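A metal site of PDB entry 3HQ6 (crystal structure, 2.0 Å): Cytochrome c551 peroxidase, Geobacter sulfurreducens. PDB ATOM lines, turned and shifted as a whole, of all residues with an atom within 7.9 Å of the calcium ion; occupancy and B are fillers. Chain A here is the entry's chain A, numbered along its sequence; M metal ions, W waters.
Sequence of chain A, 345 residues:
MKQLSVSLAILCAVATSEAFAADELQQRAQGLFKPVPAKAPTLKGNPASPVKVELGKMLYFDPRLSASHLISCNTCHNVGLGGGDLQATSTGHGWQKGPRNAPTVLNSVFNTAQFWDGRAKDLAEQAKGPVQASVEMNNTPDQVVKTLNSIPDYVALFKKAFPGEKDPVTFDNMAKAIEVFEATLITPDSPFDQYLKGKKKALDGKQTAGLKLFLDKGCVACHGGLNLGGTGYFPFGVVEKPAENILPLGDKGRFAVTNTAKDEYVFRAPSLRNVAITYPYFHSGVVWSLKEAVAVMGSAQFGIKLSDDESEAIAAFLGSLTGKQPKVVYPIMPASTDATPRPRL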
ATOM      1  N   GLY A  84      19.026  18.359  19.817  1.00  0.00           N
ATOM      2  CA  GLY A  84      20.065  17.344  19.400  1.00  0.00           C
ATOM      3  C   GLY A  84      19.408  15.970  19.323  1.00  0.00           C
ATOM      4  O   GLY A  84      18.213  15.880  19.055  1.00  0.00           O
ATOM      5  N   ASP A  85      20.198  14.874  19.472  1.00  0.00           N
ATOM      6  CA  ASP A  85      19.662  13.486  19.304  1.00  0.00           C
ATOM      7  C   ASP A  85      19.976  12.458  20.389  1.00  0.00           C
ATOM      8  O   ASP A  85      19.581  11.296  20.245  1.00  0.00           O
ATOM      9  CB  ASP A  85      20.108  12.890  17.961  1.00  0.00           C
ATOM     10  CG  ASP A  85      21.621  12.672  17.880  1.00  0.00           C
ATOM     11  OD1 ASP A  85      22.339  12.777  18.895  1.00  0.00           O
ATOM     12  OD2 ASP A  85      22.117  12.398  16.778  1.00  0.00           O
ATOM     13  N   LEU A  86      20.708  12.849  21.437  1.00  0.00           N
ATOM     14  CA  LEU A  86      21.043  11.983  22.596  1.00  0.00           C
ATOM     15  C   LEU A  86      22.099  10.855  22.317  1.00  0.00           C
ATOM     16  O   LEU A  86      22.115   9.887  23.037  1.00  0.00           O
ATOM     17  CB  LEU A  86      19.758  11.276  23.146  1.00  0.00           C
ATOM     18  CG  LEU A  86      18.399  11.937  23.607  1.00  0.00           C
ATOM     19  CD1 LEU A  86      17.204  10.881  23.460  1.00  0.00           C
ATOM     20  CD2 LEU A  86      18.479  12.445  24.999  1.00  0.00           C
ATOM     21  N   GLN A  87      22.891  10.973  21.262  1.00  0.00           N
ATOM     22  CA  GLN A  87      23.796   9.969  20.788  1.00  0.00           C
ATOM     23  C   GLN A  87      25.239  10.432  20.889  1.00  0.00           C
ATOM     24  O   GLN A  87      25.517  11.625  20.842  1.00  0.00           O
ATOM     25  CB  GLN A  87      23.439   9.611  19.342  1.00  0.00           C
ATOM     26  CG  GLN A  87      22.070   8.980  19.171  1.00  0.00           C
ATOM     27  CD  GLN A  87      21.887   7.544  19.761  1.00  0.00           C
ATOM     28  OE1 GLN A  87      22.814   6.722  19.867  1.00  0.00           O
ATOM     29  NE2 GLN A  87      20.689   7.267  20.164  1.00  0.00           N
ATOM     30  N   ALA A  88      26.209   9.516  20.956  1.00  0.00           N
ATOM     31  CA  ALA A  88      27.588   9.986  21.050  1.00  0.00           C
ATOM     32  C   ALA A  88      27.956  10.765  19.754  1.00  0.00           C
ATOM     33  O   ALA A  88      28.340  11.961  19.810  1.00  0.00           O
ATOM     34  CB  ALA A  88      28.601   8.792  21.377  1.00  0.00           C
ATOM     35  N   ASN A 101      29.317  14.434  17.048  1.00  0.00           N
ATOM     36  CA  ASN A 101      28.155  14.627  17.927  1.00  0.00           C
ATOM     37  C   ASN A 101      27.278  15.669  17.228  1.00  0.00           C
ATOM     38  O   ASN A 101      27.822  16.728  16.857  1.00  0.00           O
ATOM     39  CB  ASN A 101      28.605  15.167  19.330  1.00  0.00           C
ATOM     40  CG  ASN A 101      27.460  15.285  20.280  1.00  0.00           C
ATOM     41  OD1 ASN A 101      27.003  16.428  20.631  1.00  0.00           O
ATOM     42  ND2 ASN A 101      26.957  14.106  20.731  1.00  0.00           N
ATOM     43  N   ALA A 102      25.988  15.382  16.963  1.00  0.00           N
ATOM     44  CA  ALA A 102      25.113  16.410  16.387  1.00  0.00           C
ATOM     45  C   ALA A 102      24.939  17.619  17.307  1.00  0.00           C
ATOM     46  O   ALA A 102      24.403  17.503  18.396  1.00  0.00           O
ATOM     47  CB  ALA A 102      23.712  15.804  15.924  1.00  0.00           C
ATOM     48  N   PRO A 103      25.402  18.804  16.853  1.00  0.00           N
ATOM     49  CA  PRO A 103      25.043  20.028  17.592  1.00  0.00           C
ATOM     50  C   PRO A 103      23.560  20.303  17.557  1.00  0.00           C
ATOM     51  O   PRO A 103      22.845  19.904  16.607  1.00  0.00           O
ATOM     52  CB  PRO A 103      25.740  21.122  16.813  1.00  0.00           C
ATOM     53  CG  PRO A 103      25.661  20.578  15.340  1.00  0.00           C
ATOM     54  CD  PRO A 103      26.071  19.118  15.563  1.00  0.00           C
ATOM     55  N   THR A 104      23.101  21.065  18.526  1.00  0.00           N
ATOM     56  CA  THR A 104      21.712  21.478  18.587  1.00  0.00           C
ATOM     57  C   THR A 104      21.319  22.457  17.374  1.00  0.00           C
ATOM     58  O   THR A 104      22.068  23.347  16.989  1.00  0.00           O
ATOM     59  CB  THR A 104      21.451  22.125  19.975  1.00  0.00           C
ATOM     60  OG1 THR A 104      20.085  22.410  20.089  1.00  0.00           O
ATOM     61  CG2 THR A 104      22.205  23.434  20.134  1.00  0.00           C
ATOM     62  N   TRP A 116      32.388  21.284  12.759  1.00  0.00           N
ATOM     63  CA  TRP A 116      33.058  20.841  14.037  1.00  0.00           C
ATOM     64  C   TRP A 116      34.565  21.043  14.028  1.00  0.00           C
ATOM     65  O   TRP A 116      35.163  21.421  15.015  1.00  0.00           O
ATOM     66  CB  TRP A 116      32.759  19.380  14.399  1.00  0.00           C
ATOM     67  CG  TRP A 116      31.743  19.137  15.479  1.00  0.00           C
ATOM     68  CD1 TRP A 116      30.554  18.500  15.338  1.00  0.00           C
ATOM     69  CD2 TRP A 116      31.845  19.482  16.877  1.00  0.00           C
ATOM     70  NE1 TRP A 116      29.862  18.481  16.536  1.00  0.00           N
ATOM     71  CE2 TRP A 116      30.639  19.065  17.495  1.00  0.00           C
ATOM     72  CE3 TRP A 116      32.815  20.171  17.660  1.00  0.00           C
ATOM     73  CZ2 TRP A 116      30.387  19.244  18.865  1.00  0.00           C
ATOM     74  CZ3 TRP A 116      32.563  20.330  19.076  1.00  0.00           C
ATOM     75  CH2 TRP A 116      31.350  19.864  19.628  1.00  0.00           C
ATOM     76  N   VAL A 275      23.421  24.054  26.934  1.00  0.00           N
ATOM     77  CA  VAL A 275      24.415  22.920  27.136  1.00  0.00           C
ATOM     78  C   VAL A 275      23.872  21.855  28.144  1.00  0.00           C
ATOM     79  O   VAL A 275      24.106  20.650  27.983  1.00  0.00           O
ATOM     80  CB  VAL A 275      25.776  23.433  27.513  1.00  0.00           C
ATOM     81  CG1 VAL A 275      25.780  24.091  28.869  1.00  0.00           C
ATOM     82  CG2 VAL A 275      26.893  22.212  27.458  1.00  0.00           C
ATOM     83  N   ILE A 277      21.217  20.442  28.345  1.00  0.00           N
ATOM     84  CA  ILE A 277      20.230  19.492  27.769  1.00  0.00           C
ATOM     85  C   ILE A 277      20.681  18.930  26.436  1.00  0.00           C
ATOM     86  O   ILE A 277      19.923  18.284  25.752  1.00  0.00           O
ATOM     87  CB  ILE A 277      18.794  20.089  27.623  1.00  0.00           C
ATOM     88  CG1 ILE A 277      18.743  21.173  26.552  1.00  0.00           C
ATOM     89  CG2 ILE A 277      18.323  20.630  28.924  1.00  0.00           C
ATOM     90  CD1 ILE A 277      17.441  22.004  26.453  1.00  0.00           C
ATOM     91  N   THR A 278      21.950  19.140  26.082  1.00  0.00           N
ATOM     92  CA  THR A 278      22.447  18.599  24.799  1.00  0.00           C
ATOM     93  C   THR A 278      23.642  17.670  25.014  1.00  0.00           C
ATOM     94  O   THR A 278      24.532  17.549  24.179  1.00  0.00           O
ATOM     95  CB  THR A 278      22.800  19.702  23.837  1.00  0.00           C
ATOM     96  OG1 THR A 278      23.913  20.398  24.375  1.00  0.00           O
ATOM     97  CG2 THR A 278      21.596  20.781  23.673  1.00  0.00           C
ATOM     98  N   TYR A 279      23.650  16.980  26.149  1.00  0.00           N
ATOM     99  CA  TYR A 279      24.601  15.917  26.384  1.00  0.00           C
ATOM    100  C   TYR A 279      24.416  14.876  25.317  1.00  0.00           C
ATOM    101  O   TYR A 279      23.379  14.802  24.679  1.00  0.00           O
ATOM    102  CB  TYR A 279      24.337  15.287  27.724  1.00  0.00           C
ATOM    103  CG  TYR A 279      22.861  15.011  27.915  1.00  0.00           C
ATOM    104  CD1 TYR A 279      22.284  13.823  27.409  1.00  0.00           C
ATOM    105  CD2 TYR A 279      22.058  15.935  28.557  1.00  0.00           C
ATOM    106  CE1 TYR A 279      20.954  13.586  27.501  1.00  0.00           C
ATOM    107  CE2 TYR A 279      20.680  15.691  28.663  1.00  0.00           C
ATOM    108  CZ  TYR A 279      20.185  14.522  28.145  1.00  0.00           C
ATOM    109  OH  TYR A 279      18.883  14.262  28.215  1.00  0.00           O
ATOM    110  N   PRO A 280      25.413  14.040  25.108  1.00  0.00           N
ATOM    111  CA  PRO A 280      26.750  14.094  25.671  1.00  0.00           C
ATOM    112  C   PRO A 280      27.655  15.152  24.972  1.00  0.00           C
ATOM    113  O   PRO A 280      27.222  15.854  24.020  1.00  0.00           O
ATOM    114  CB  PRO A 280      27.266  12.681  25.455  1.00  0.00           C
ATOM    115  CG  PRO A 280      26.576  12.221  24.222  1.00  0.00           C
ATOM    116  CD  PRO A 280      25.199  12.862  24.266  1.00  0.00           C
ATOM    117  N   TYR A 281      28.871  15.295  25.453  1.00  0.00           N
ATOM    118  CA  TYR A 281      29.675  16.499  25.138  1.00  0.00           C
ATOM    119  C   TYR A 281      30.924  16.238  24.369  1.00  0.00           C
ATOM    120  O   TYR A 281      31.441  15.060  24.329  1.00  0.00           O
ATOM    121  CB  TYR A 281      29.989  17.311  26.399  1.00  0.00           C
ATOM    122  CG  TYR A 281      28.789  17.600  27.159  1.00  0.00           C
ATOM    123  CD1 TYR A 281      27.856  18.581  26.695  1.00  0.00           C
ATOM    124  CD2 TYR A 281      28.506  16.877  28.303  1.00  0.00           C
ATOM    125  CE1 TYR A 281      26.695  18.825  27.348  1.00  0.00           C
ATOM    126  CE2 TYR A 281      27.297  17.106  29.006  1.00  0.00           C
ATOM    127  CZ  TYR A 281      26.419  18.117  28.525  1.00  0.00           C
ATOM    128  OH  TYR A 281      25.242  18.387  29.184  1.00  0.00           O
ATOM    129  N   PHE A 282      31.364  17.317  23.714  1.00  0.00           N
ATOM    130  CA  PHE A 282      32.525  17.375  22.737  1.00  0.00           C
ATOM    131  C   PHE A 282      32.200  16.734  21.366  1.00  0.00           C
ATOM    132  O   PHE A 282      31.118  16.155  21.164  1.00  0.00           O
ATOM    133  CB  PHE A 282      33.847  16.848  23.354  1.00  0.00           C
ATOM    134  CG  PHE A 282      34.120  17.450  24.742  1.00  0.00           C
ATOM    135  CD1 PHE A 282      34.269  18.852  24.896  1.00  0.00           C
ATOM    136  CD2 PHE A 282      34.237  16.608  25.873  1.00  0.00           C
ATOM    137  CE1 PHE A 282      34.520  19.450  26.180  1.00  0.00           C
ATOM    138  CE2 PHE A 282      34.475  17.103  27.126  1.00  0.00           C
ATOM    139  CZ  PHE A 282      34.643  18.567  27.307  1.00  0.00           C
ATOM    140  N   HIS A 283      33.117  16.895  20.435  1.00  0.00           N
ATOM    141  CA  HIS A 283      32.896  16.558  19.029  1.00  0.00           C
ATOM    142  C   HIS A 283      32.644  15.073  18.845  1.00  0.00           C
ATOM    143  O   HIS A 283      32.014  14.673  17.892  1.00  0.00           O
ATOM    144  CB  HIS A 283      34.113  17.032  18.217  1.00  0.00           C
ATOM    145  CG  HIS A 283      35.304  16.176  18.432  1.00  0.00           C
ATOM    146  ND1 HIS A 283      36.271  16.476  19.356  1.00  0.00           N
ATOM    147  CD2 HIS A 283      35.698  15.006  17.855  1.00  0.00           C
ATOM    148  CE1 HIS A 283      37.208  15.533  19.344  1.00  0.00           C
ATOM    149  NE2 HIS A 283      36.870  14.616  18.468  1.00  0.00           N
ATOM    150  N   SER A 284      33.175  14.277  19.759  1.00  0.00           N
ATOM    151  CA  SER A 284      33.051  12.820  19.786  1.00  0.00           C
ATOM    152  C   SER A 284      31.968  12.311  20.786  1.00  0.00           C
ATOM    153  O   SER A 284      31.703  11.071  20.857  1.00  0.00           O
ATOM    154  CB  SER A 284      34.423  12.202  20.156  1.00  0.00           C
ATOM    155  OG  SER A 284      34.851  12.861  21.355  1.00  0.00           O
ATOM    156  N   GLY A 285      31.269  13.224  21.489  1.00  0.00           N
ATOM    157  CA  GLY A 285      30.223  12.768  22.414  1.00  0.00           C
ATOM    158  C   GLY A 285      30.633  11.811  23.545  1.00  0.00           C
ATOM    159  O   GLY A 285      29.841  10.993  23.964  1.00  0.00           O
ATOM    160  N   VAL A 287      31.874  12.513  26.829  1.00  0.00           N
ATOM    161  CA  VAL A 287      31.639  12.859  28.209  1.00  0.00           C
ATOM    162  C   VAL A 287      30.183  13.090  28.346  1.00  0.00           C
ATOM    163  O   VAL A 287      29.627  13.977  27.683  1.00  0.00           O
ATOM    164  CB  VAL A 287      32.446  14.101  28.704  1.00  0.00           C
ATOM    165  CG1 VAL A 287      32.024  14.466  30.154  1.00  0.00           C
ATOM    166  CG2 VAL A 287      33.900  13.843  28.684  1.00  0.00           C
HETATM  167 CA    CA M   1      26.158  17.334  22.504  1.00  0.00          CA
HETATM  168  O   HOH W   1      24.575  15.655  21.906  1.00  0.00           O
HETATM  169  O   HOH W   2      24.881  18.484  20.938  1.00  0.00           O
HETATM  170  O   HOH W   3      28.505  18.292  21.985  1.00  0.00           O
HETATM  171  O   HOH W   4      26.422  19.433  23.590  1.00  0.00           O
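The backbone NH of Asn 101 lies within hydrogen-bond range of the backbone carbonyl oxygen of His 283 (2.8 Å).
O of Ala 88 sits at hydrogen-bond distance from ND2 of Asn 101.
O of Gln 87 is in hydrogen-bond range of ND2 of Asn 101 (2.9 Å).
The indole nitrogen (NE1) of Trp 116 sits at hydrogen-bond distance from the backbone carbonyl oxygen (O) of Asn 101 (2.7 Å).
Within 4 Å of the calcium ion: Asn 101, Thr 278 and Pro 280.
The nearest printed residue that does not touch the calcium ion is Tyr 279 (4.1 Å).
The calcium ion is bound by the side-chain amide oxygen of Asn 101 (2.2 Å), water W2 (2.3 Å), the backbone carbonyl oxygen of Thr 278 (2.3 Å), the backbone carbonyl oxygen of Pro 280 (2.4 Å), water W4 (2.4 Å), water W1 (2.4 Å) and water W3 (2.6 Å).
Water W1 bridges the side-chain amide nitrogen of Asn 101 (3.1 Å) and the backbone carbonyl oxygen of Tyr 279 (3.1 Å).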
